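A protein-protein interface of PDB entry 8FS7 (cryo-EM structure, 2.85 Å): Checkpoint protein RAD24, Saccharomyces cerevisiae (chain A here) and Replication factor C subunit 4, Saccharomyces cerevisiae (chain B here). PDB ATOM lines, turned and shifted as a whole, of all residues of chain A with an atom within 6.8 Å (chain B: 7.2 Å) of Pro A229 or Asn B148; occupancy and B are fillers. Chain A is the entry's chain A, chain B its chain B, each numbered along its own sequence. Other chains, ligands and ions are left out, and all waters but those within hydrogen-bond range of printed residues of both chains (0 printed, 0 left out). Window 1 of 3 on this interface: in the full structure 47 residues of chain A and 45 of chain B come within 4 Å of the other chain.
OE2 of Glu B152 sits close to N of Thr A336, 3.5 Å away.
The side-chain amino group (NZ) of Lys B149 is in hydrogen-bond range of the side-chain amide oxygen (OE1) of Gln B146 (3.1 Å).
The side-chain amide nitrogen of Asn A366 lies within hydrogen-bond range of the side-chain carboxylate of Glu A334 (2.9 Å).
The side-chain amide oxygen (OD1) of Asn A369 sits close to the side-chain carboxylate (OE2) of Glu A230 (3.5 Å).
N of Ile B151 sits at hydrogen-bond distance from OE1 of Gln B124.
OD1 of Asn A366 sits close to OE1 of Glu A365, 2.9 Å away.
Among the printed residues, pairs that only touch across the chains: Pro A229 with Asn B148, Pro A229 with Lys B149, Pro A229 with Ile B151, Glu A230 with Lys B149, Glu A365 with Asn B148 and Asn A366 with Asn B148.
Of chain B, only Asn B148 (3.3 Å), Lys B149 (3.3 Å) and Ile B151 (3.9 Å) come within 4 Å of Pro A229.
Tyr A242 touches none of the printed residues of chain B.
Ser B147 touches none of the printed residues of chain A.
Of the printed residues of chain A, Asn B148 touches Pro A229, Glu A365 and Asn A366.
Of the printed residues of chain A, Lys B149 touches Pro A229 (3.3 Å) and Glu A230 (3.3 Å).
Of the printed residues of chain A, Ile B151 touches Pro A229 (3.9 Å).
Hydrophobic or aromatic side chains of chain A within 4 Å of the printed part of chain B: Pro A229.
Along chain A the printed residues that touch a printed residue of chain B span positions 229 to 366.
Of the 16 printed residues of chain B, 4 touch a printed residue of chain A.
Printed residues of chain B that touch a printed residue of chain A: Asn B148, Lys B149, Ile B151 and Glu B152.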
ATOM      1  N   GLU A 227      14.639  -1.275   6.005  1.00  0.00           N
ATOM      2  CA  GLU A 227      14.757  -2.181   4.871  1.00  0.00           C
ATOM      3  C   GLU A 227      16.217  -2.583   4.700  1.00  0.00           C
ATOM      4  O   GLU A 227      17.087  -1.722   4.522  1.00  0.00           O
ATOM      5  CB  GLU A 227      14.225  -1.526   3.597  1.00  0.00           C
ATOM      6  CG  GLU A 227      12.959  -0.714   3.803  1.00  0.00           C
ATOM      7  CD  GLU A 227      11.700  -1.546   3.661  1.00  0.00           C
ATOM      8  OE1 GLU A 227      11.794  -2.688   3.163  1.00  0.00           O
ATOM      9  OE2 GLU A 227      10.617  -1.057   4.045  1.00  0.00           O
ATOM     10  N   ILE A 228      16.484  -3.883   4.756  1.00  0.00           N
ATOM     11  CA  ILE A 228      17.840  -4.399   4.599  1.00  0.00           C
ATOM     12  C   ILE A 228      18.224  -4.323   3.126  1.00  0.00           C
ATOM     13  O   ILE A 228      17.537  -4.908   2.276  1.00  0.00           O
ATOM     14  CB  ILE A 228      17.959  -5.835   5.135  1.00  0.00           C
ATOM     15  CG1 ILE A 228      17.879  -5.852   6.665  1.00  0.00           C
ATOM     16  CG2 ILE A 228      19.259  -6.472   4.668  1.00  0.00           C
ATOM     17  CD1 ILE A 228      18.549  -4.672   7.344  1.00  0.00           C
ATOM     18  N   PRO A 229      19.293  -3.615   2.779  1.00  0.00           N
ATOM     19  CA  PRO A 229      19.703  -3.532   1.374  1.00  0.00           C
ATOM     20  C   PRO A 229      20.239  -4.863   0.869  1.00  0.00           C
ATOM     21  O   PRO A 229      20.648  -5.736   1.638  1.00  0.00           O
ATOM     22  CB  PRO A 229      20.798  -2.459   1.381  1.00  0.00           C
ATOM     23  CG  PRO A 229      20.628  -1.736   2.691  1.00  0.00           C
ATOM     24  CD  PRO A 229      20.128  -2.768   3.644  1.00  0.00           C
ATOM     25  N   GLU A 230      20.221  -5.009  -0.454  1.00  0.00           N
ATOM     26  CA  GLU A 230      20.706  -6.231  -1.079  1.00  0.00           C
ATOM     27  C   GLU A 230      22.203  -6.398  -0.842  1.00  0.00           C
ATOM     28  O   GLU A 230      22.985  -5.461  -1.030  1.00  0.00           O
ATOM     29  CB  GLU A 230      20.395  -6.218  -2.578  1.00  0.00           C
ATOM     30  CG  GLU A 230      20.855  -4.966  -3.313  1.00  0.00           C
ATOM     31  CD  GLU A 230      19.745  -3.947  -3.485  1.00  0.00           C
ATOM     32  OE1 GLU A 230      19.604  -3.065  -2.612  1.00  0.00           O
ATOM     33  OE2 GLU A 230      19.014  -4.027  -4.495  1.00  0.00           O
ATOM     34  N   ASN A 231      22.597  -7.596  -0.409  1.00  0.00           N
ATOM     35  CA  ASN A 231      23.995  -7.894  -0.117  1.00  0.00           C
ATOM     36  C   ASN A 231      24.534  -9.012  -1.000  1.00  0.00           C
ATOM     37  O   ASN A 231      25.586  -8.843  -1.626  1.00  0.00           O
ATOM     38  CB  ASN A 231      24.154  -8.248   1.368  1.00  0.00           C
ATOM     39  CG  ASN A 231      25.582  -8.103   1.853  1.00  0.00           C
ATOM     40  OD1 ASN A 231      26.431  -7.539   1.162  1.00  0.00           O
ATOM     41  ND2 ASN A 231      25.855  -8.613   3.048  1.00  0.00           N
ATOM     42  N   ASP A 232      23.846 -10.148  -1.071  1.00  0.00           N
ATOM     43  CA  ASP A 232      24.276 -11.287  -1.865  1.00  0.00           C
ATOM     44  C   ASP A 232      23.195 -11.652  -2.875  1.00  0.00           C
ATOM     45  O   ASP A 232      22.009 -11.378  -2.673  1.00  0.00           O
ATOM     46  CB  ASP A 232      24.599 -12.496  -0.976  1.00  0.00           C
ATOM     47  CG  ASP A 232      25.816 -12.267  -0.099  1.00  0.00           C
ATOM     48  OD1 ASP A 232      26.560 -11.296  -0.351  1.00  0.00           O
ATOM     49  OD2 ASP A 232      26.026 -13.057   0.845  1.00  0.00           O
ATOM     50  N   LYS A 237      16.277 -15.570  -0.798  1.00  0.00           N
ATOM     51  CA  LYS A 237      16.130 -14.454   0.127  1.00  0.00           C
ATOM     52  C   LYS A 237      14.896 -14.648   0.998  1.00  0.00           C
ATOM     53  O   LYS A 237      13.827 -15.023   0.508  1.00  0.00           O
ATOM     54  CB  LYS A 237      16.031 -13.142  -0.651  1.00  0.00           C
ATOM     55  CG  LYS A 237      17.362 -12.456  -0.915  1.00  0.00           C
ATOM     56  CD  LYS A 237      17.148 -11.060  -1.481  1.00  0.00           C
ATOM     57  CE  LYS A 237      18.442 -10.262  -1.504  1.00  0.00           C
ATOM     58  NZ  LYS A 237      19.499 -10.941  -2.304  1.00  0.00           N
ATOM     59  N   ASP A 241      15.957 -11.160   5.252  1.00  0.00           N
ATOM     60  CA  ASP A 241      16.926 -10.691   4.267  1.00  0.00           C
ATOM     61  C   ASP A 241      16.406  -9.474   3.510  1.00  0.00           C
ATOM     62  O   ASP A 241      17.186  -8.586   3.147  1.00  0.00           O
ATOM     63  CB  ASP A 241      17.279 -11.819   3.298  1.00  0.00           C
ATOM     64  CG  ASP A 241      18.064 -12.932   3.964  1.00  0.00           C
ATOM     65  OD1 ASP A 241      18.719 -12.665   4.994  1.00  0.00           O
ATOM     66  OD2 ASP A 241      18.026 -14.073   3.457  1.00  0.00           O
ATOM     67  N   TYR A 242      15.097  -9.412   3.263  1.00  0.00           N
ATOM     68  CA  TYR A 242      14.539  -8.264   2.555  1.00  0.00           C
ATOM     69  C   TYR A 242      14.429  -7.045   3.464  1.00  0.00           C
ATOM     70  O   TYR A 242      15.045  -6.007   3.199  1.00  0.00           O
ATOM     71  CB  TYR A 242      13.169  -8.610   1.966  1.00  0.00           C
ATOM     72  CG  TYR A 242      13.217  -9.185   0.568  1.00  0.00           C
ATOM     73  CD1 TYR A 242      13.282  -8.353  -0.543  1.00  0.00           C
ATOM     74  CD2 TYR A 242      13.208 -10.556   0.358  1.00  0.00           C
ATOM     75  CE1 TYR A 242      13.329  -8.871  -1.823  1.00  0.00           C
ATOM     76  CE2 TYR A 242      13.248 -11.083  -0.918  1.00  0.00           C
ATOM     77  CZ  TYR A 242      13.312 -10.237  -2.005  1.00  0.00           C
ATOM     78  OH  TYR A 242      13.357 -10.760  -3.276  1.00  0.00           O
ATOM     79  N   GLU A 334      17.534   9.754   3.496  1.00  0.00           N
ATOM     80  CA  GLU A 334      16.329   9.479   2.726  1.00  0.00           C
ATOM     81  C   GLU A 334      15.641   8.233   3.266  1.00  0.00           C
ATOM     82  O   GLU A 334      16.231   7.148   3.288  1.00  0.00           O
ATOM     83  CB  GLU A 334      16.665   9.301   1.245  1.00  0.00           C
ATOM     84  CG  GLU A 334      15.462   9.393   0.321  1.00  0.00           C
ATOM     85  CD  GLU A 334      15.857   9.531  -1.136  1.00  0.00           C
ATOM     86  OE1 GLU A 334      17.033   9.268  -1.463  1.00  0.00           O
ATOM     87  OE2 GLU A 334      14.990   9.904  -1.955  1.00  0.00           O
ATOM     88  N   THR A 336      12.998   5.135   3.299  1.00  0.00           N
ATOM     89  CA  THR A 336      12.489   4.223   2.287  1.00  0.00           C
ATOM     90  C   THR A 336      10.978   4.370   2.143  1.00  0.00           C
ATOM     91  O   THR A 336      10.278   4.795   3.066  1.00  0.00           O
ATOM     92  CB  THR A 336      12.840   2.778   2.638  1.00  0.00           C
ATOM     93  OG1 THR A 336      12.766   2.598   4.059  1.00  0.00           O
ATOM     94  CG2 THR A 336      14.245   2.441   2.160  1.00  0.00           C
ATOM     95  N   GLU A 365      15.497   3.278  -8.175  1.00  0.00           N
ATOM     96  CA  GLU A 365      16.846   3.431  -7.644  1.00  0.00           C
ATOM     97  C   GLU A 365      16.884   3.333  -6.124  1.00  0.00           C
ATOM     98  O   GLU A 365      17.857   2.815  -5.566  1.00  0.00           O
ATOM     99  CB  GLU A 365      17.436   4.767  -8.102  1.00  0.00           C
ATOM    100  CG  GLU A 365      18.905   4.956  -7.760  1.00  0.00           C
ATOM    101  CD  GLU A 365      19.154   6.205  -6.938  1.00  0.00           C
ATOM    102  OE1 GLU A 365      18.275   7.091  -6.920  1.00  0.00           O
ATOM    103  OE2 GLU A 365      20.230   6.299  -6.310  1.00  0.00           O
ATOM    104  N   ASN A 366      15.843   3.809  -5.440  1.00  0.00           N
ATOM    105  CA  ASN A 366      15.835   3.848  -3.983  1.00  0.00           C
ATOM    106  C   ASN A 366      15.155   2.647  -3.342  1.00  0.00           C
ATOM    107  O   ASN A 366      15.524   2.268  -2.225  1.00  0.00           O
ATOM    108  CB  ASN A 366      15.147   5.128  -3.494  1.00  0.00           C
ATOM    109  CG  ASN A 366      15.910   6.381  -3.874  1.00  0.00           C
ATOM    110  OD1 ASN A 366      17.032   6.310  -4.375  1.00  0.00           O
ATOM    111  ND2 ASN A 366      15.303   7.538  -3.639  1.00  0.00           N
ATOM    112  N   SER A 367      14.178   2.040  -4.009  1.00  0.00           N
ATOM    113  CA  SER A 367      13.401   0.937  -3.451  1.00  0.00           C
ATOM    114  C   SER A 367      13.364  -0.235  -4.422  1.00  0.00           C
ATOM    115  O   SER A 367      12.309  -0.802  -4.716  1.00  0.00           O
ATOM    116  CB  SER A 367      11.987   1.393  -3.099  1.00  0.00           C
ATOM    117  OG  SER A 367      11.272   1.778  -4.260  1.00  0.00           O
ATOM    118  N   ASN A 369      14.514  -3.190  -3.918  1.00  0.00           N
ATOM    119  CA  ASN A 369      14.203  -4.437  -3.224  1.00  0.00           C
ATOM    120  C   ASN A 369      12.705  -4.712  -3.222  1.00  0.00           C
ATOM    121  O   ASN A 369      12.272  -5.848  -3.448  1.00  0.00           O
ATOM    122  CB  ASN A 369      14.741  -4.388  -1.794  1.00  0.00           C
ATOM    123  CG  ASN A 369      15.928  -5.307  -1.587  1.00  0.00           C
ATOM    124  OD1 ASN A 369      16.632  -5.656  -2.534  1.00  0.00           O
ATOM    125  ND2 ASN A 369      16.155  -5.707  -0.341  1.00  0.00           N
ATOM    126  N   SER B  48      29.072   9.733  -0.463  1.00  0.00           N
ATOM    127  CA  SER B  48      28.570   8.923  -1.562  1.00  0.00           C
ATOM    128  C   SER B  48      28.725   9.690  -2.867  1.00  0.00           C
ATOM    129  O   SER B  48      28.772  10.922  -2.887  1.00  0.00           O
ATOM    130  CB  SER B  48      27.102   8.530  -1.349  1.00  0.00           C
ATOM    131  OG  SER B  48      26.238   9.365  -2.099  1.00  0.00           O
ATOM    132  N   ASP B 117      29.215   0.089   1.526  1.00  0.00           N
ATOM    133  CA  ASP B 117      28.043  -0.459   0.856  1.00  0.00           C
ATOM    134  C   ASP B 117      28.064  -1.980   0.774  1.00  0.00           C
ATOM    135  O   ASP B 117      27.018  -2.580   0.506  1.00  0.00           O
ATOM    136  CB  ASP B 117      27.926   0.127  -0.551  1.00  0.00           C
ATOM    137  CG  ASP B 117      29.265   0.229  -1.255  1.00  0.00           C
ATOM    138  OD1 ASP B 117      29.805  -0.821  -1.662  1.00  0.00           O
ATOM    139  OD2 ASP B 117      29.776   1.358  -1.404  1.00  0.00           O
ATOM    140  N   MET B 119      28.962  -4.148   3.299  1.00  0.00           N
ATOM    141  CA  MET B 119      29.074  -4.692   4.645  1.00  0.00           C
ATOM    142  C   MET B 119      27.779  -5.393   5.038  1.00  0.00           C
ATOM    143  O   MET B 119      26.684  -4.939   4.692  1.00  0.00           O
ATOM    144  CB  MET B 119      29.403  -3.586   5.650  1.00  0.00           C
ATOM    145  CG  MET B 119      29.923  -4.096   6.982  1.00  0.00           C
ATOM    146  SD  MET B 119      30.530  -2.803   8.085  1.00  0.00           S
ATOM    147  CE  MET B 119      30.561  -1.381   6.995  1.00  0.00           C
ATOM    148  N   ALA B 121      24.621  -6.851   7.217  1.00  0.00           N
ATOM    149  CA  ALA B 121      23.668  -6.107   8.039  1.00  0.00           C
ATOM    150  C   ALA B 121      23.946  -6.277   9.529  1.00  0.00           C
ATOM    151  O   ALA B 121      23.782  -5.328  10.307  1.00  0.00           O
ATOM    152  CB  ALA B 121      22.243  -6.542   7.704  1.00  0.00           C
ATOM    153  N   GLN B 124      26.361  -3.920  10.469  1.00  0.00           N
ATOM    154  CA  GLN B 124      25.752  -2.598  10.586  1.00  0.00           C
ATOM    155  C   GLN B 124      25.099  -2.405  11.952  1.00  0.00           C
ATOM    156  O   GLN B 124      25.215  -1.332  12.555  1.00  0.00           O
ATOM    157  CB  GLN B 124      24.732  -2.382   9.466  1.00  0.00           C
ATOM    158  CG  GLN B 124      25.230  -2.770   8.083  1.00  0.00           C
ATOM    159  CD  GLN B 124      25.297  -1.596   7.125  1.00  0.00           C
ATOM    160  OE1 GLN B 124      24.586  -0.607   7.288  1.00  0.00           O
ATOM    161  NE2 GLN B 124      26.155  -1.704   6.118  1.00  0.00           N
ATOM    162  N   CYS B 144      31.223   5.350   0.339  1.00  0.00           N
ATOM    163  CA  CYS B 144      30.365   4.431  -0.393  1.00  0.00           C
ATOM    164  C   CYS B 144      30.023   5.034  -1.747  1.00  0.00           C
ATOM    165  O   CYS B 144      30.279   6.211  -2.010  1.00  0.00           O
ATOM    166  CB  CYS B 144      29.090   4.114   0.396  1.00  0.00           C
ATOM    167  SG  CYS B 144      28.097   5.568   0.806  1.00  0.00           S
ATOM    168  N   ASN B 145      29.443   4.203  -2.611  1.00  0.00           N
ATOM    169  CA  ASN B 145      28.963   4.663  -3.908  1.00  0.00           C
ATOM    170  C   ASN B 145      27.508   5.112  -3.849  1.00  0.00           C
ATOM    171  O   ASN B 145      27.133   6.087  -4.510  1.00  0.00           O
ATOM    172  CB  ASN B 145      29.129   3.559  -4.954  1.00  0.00           C
ATOM    173  CG  ASN B 145      30.555   3.439  -5.454  1.00  0.00           C
ATOM    174  OD1 ASN B 145      31.082   2.338  -5.605  1.00  0.00           O
ATOM    175  ND2 ASN B 145      31.188   4.578  -5.713  1.00  0.00           N
ATOM    176  N   GLN B 146      26.681   4.417  -3.071  1.00  0.00           N
ATOM    177  CA  GLN B 146      25.290   4.799  -2.865  1.00  0.00           C
ATOM    178  C   GLN B 146      24.970   4.706  -1.381  1.00  0.00           C
ATOM    179  O   GLN B 146      25.376   3.749  -0.716  1.00  0.00           O
ATOM    180  CB  GLN B 146      24.340   3.911  -3.680  1.00  0.00           C
ATOM    181  CG  GLN B 146      24.602   2.420  -3.548  1.00  0.00           C
ATOM    182  CD  GLN B 146      24.273   1.658  -4.816  1.00  0.00           C
ATOM    183  OE1 GLN B 146      23.469   0.725  -4.803  1.00  0.00           O
ATOM    184  NE2 GLN B 146      24.896   2.051  -5.921  1.00  0.00           N
ATOM    185  N   SER B 147      24.249   5.703  -0.868  1.00  0.00           N
ATOM    186  CA  SER B 147      23.916   5.742   0.551  1.00  0.00           C
ATOM    187  C   SER B 147      22.778   4.801   0.922  1.00  0.00           C
ATOM    188  O   SER B 147      22.553   4.574   2.115  1.00  0.00           O
ATOM    189  CB  SER B 147      23.558   7.170   0.966  1.00  0.00           C
ATOM    190  OG  SER B 147      24.693   8.018   0.905  1.00  0.00           O
ATOM    191  N   ASN B 148      22.058   4.255  -0.062  1.00  0.00           N
ATOM    192  CA  ASN B 148      20.955   3.349   0.235  1.00  0.00           C
ATOM    193  C   ASN B 148      21.431   2.020   0.807  1.00  0.00           C
ATOM    194  O   ASN B 148      20.664   1.355   1.511  1.00  0.00           O
ATOM    195  CB  ASN B 148      20.124   3.102  -1.025  1.00  0.00           C
ATOM    196  CG  ASN B 148      20.176   4.264  -1.995  1.00  0.00           C
ATOM    197  OD1 ASN B 148      19.711   5.363  -1.692  1.00  0.00           O
ATOM    198  ND2 ASN B 148      20.746   4.029  -3.171  1.00  0.00           N
ATOM    199  N   LYS B 149      22.672   1.619   0.523  1.00  0.00           N
ATOM    200  CA  LYS B 149      23.181   0.352   1.036  1.00  0.00           C
ATOM    201  C   LYS B 149      23.508   0.415   2.522  1.00  0.00           C
ATOM    202  O   LYS B 149      23.661  -0.634   3.154  1.00  0.00           O
ATOM    203  CB  LYS B 149      24.415  -0.078   0.246  1.00  0.00           C
ATOM    204  CG  LYS B 149      24.139  -0.394  -1.213  1.00  0.00           C
ATOM    205  CD  LYS B 149      23.388  -1.706  -1.362  1.00  0.00           C
ATOM    206  CE  LYS B 149      24.043  -2.598  -2.402  1.00  0.00           C
ATOM    207  NZ  LYS B 149      24.648  -1.807  -3.510  1.00  0.00           N
ATOM    208  N   ILE B 150      23.629   1.612   3.086  1.00  0.00           N
ATOM    209  CA  ILE B 150      23.825   1.782   4.520  1.00  0.00           C
ATOM    210  C   ILE B 150      22.457   1.932   5.170  1.00  0.00           C
ATOM    211  O   ILE B 150      21.631   2.735   4.720  1.00  0.00           O
ATOM    212  CB  ILE B 150      24.724   2.994   4.814  1.00  0.00           C
ATOM    213  CG1 ILE B 150      26.176   2.679   4.450  1.00  0.00           C
ATOM    214  CG2 ILE B 150      24.637   3.388   6.277  1.00  0.00           C
ATOM    215  CD1 ILE B 150      26.592   3.191   3.091  1.00  0.00           C
ATOM    216  N   ILE B 151      22.211   1.147   6.223  1.00  0.00           N
ATOM    217  CA  ILE B 151      20.881   1.086   6.814  1.00  0.00           C
ATOM    218  C   ILE B 151      20.501   2.428   7.437  1.00  0.00           C
ATOM    219  O   ILE B 151      21.359   3.243   7.803  1.00  0.00           O
ATOM    220  CB  ILE B 151      20.802  -0.045   7.854  1.00  0.00           C
ATOM    221  CG1 ILE B 151      21.777   0.209   9.002  1.00  0.00           C
ATOM    222  CG2 ILE B 151      21.083  -1.389   7.200  1.00  0.00           C
ATOM    223  CD1 ILE B 151      21.531  -0.667  10.206  1.00  0.00           C
ATOM    224  N   GLU B 152      19.192   2.657   7.542  1.00  0.00           N
ATOM    225  CA  GLU B 152      18.685   3.930   8.053  1.00  0.00           C
ATOM    226  C   GLU B 152      19.143   4.270   9.471  1.00  0.00           C
ATOM    227  O   GLU B 152      19.467   5.448   9.708  1.00  0.00           O
ATOM    228  CB  GLU B 152      17.153   3.942   7.964  1.00  0.00           C
ATOM    229  CG  GLU B 152      16.611   3.789   6.553  1.00  0.00           C
ATOM    230  CD  GLU B 152      15.159   3.356   6.532  1.00  0.00           C
ATOM    231  OE1 GLU B 152      14.512   3.390   7.599  1.00  0.00           O
ATOM    232  OE2 GLU B 152      14.666   2.980   5.448  1.00  0.00           O
ATOM    233  N   GLN B 155      22.505   5.799   9.136  1.00  0.00           N
ATOM    234  CA  GLN B 155      22.440   7.124   8.529  1.00  0.00           C
ATOM    235  C   GLN B 155      21.829   8.161   9.461  1.00  0.00           C
ATOM    236  O   GLN B 155      22.018   9.361   9.239  1.00  0.00           O
ATOM    237  CB  GLN B 155      21.638   7.072   7.227  1.00  0.00           C
ATOM    238  CG  GLN B 155      22.121   6.032   6.236  1.00  0.00           C
ATOM    239  CD  GLN B 155      21.461   6.171   4.879  1.00  0.00           C
ATOM    240  OE1 GLN B 155      21.548   7.218   4.237  1.00  0.00           O
ATOM    241  NE2 GLN B 155      20.794   5.113   4.435  1.00  0.00           N
ATOM    242  N   ARG B 162      27.089  14.477  -0.137  1.00  0.00           N
ATOM    243  CA  ARG B 162      26.943  13.870  -1.453  1.00  0.00           C
ATOM    244  C   ARG B 162      27.929  14.516  -2.417  1.00  0.00           C
ATOM    245  O   ARG B 162      27.968  15.745  -2.544  1.00  0.00           O
ATOM    246  CB  ARG B 162      25.510  14.020  -1.964  1.00  0.00           C
ATOM    247  CG  ARG B 162      24.559  12.956  -1.442  1.00  0.00           C
ATOM    248  CD  ARG B 162      23.110  13.404  -1.551  1.00  0.00           C
ATOM    249  NE  ARG B 162      22.312  12.973  -0.408  1.00  0.00           N
ATOM    250  CZ  ARG B 162      21.887  11.732  -0.210  1.00  0.00           C
ATOM    251  NH1 ARG B 162      22.151  10.763  -1.073  1.00  0.00           N
ATOM    252  NH2 ARG B 162      21.174  11.456   0.878  1.00  0.00           N
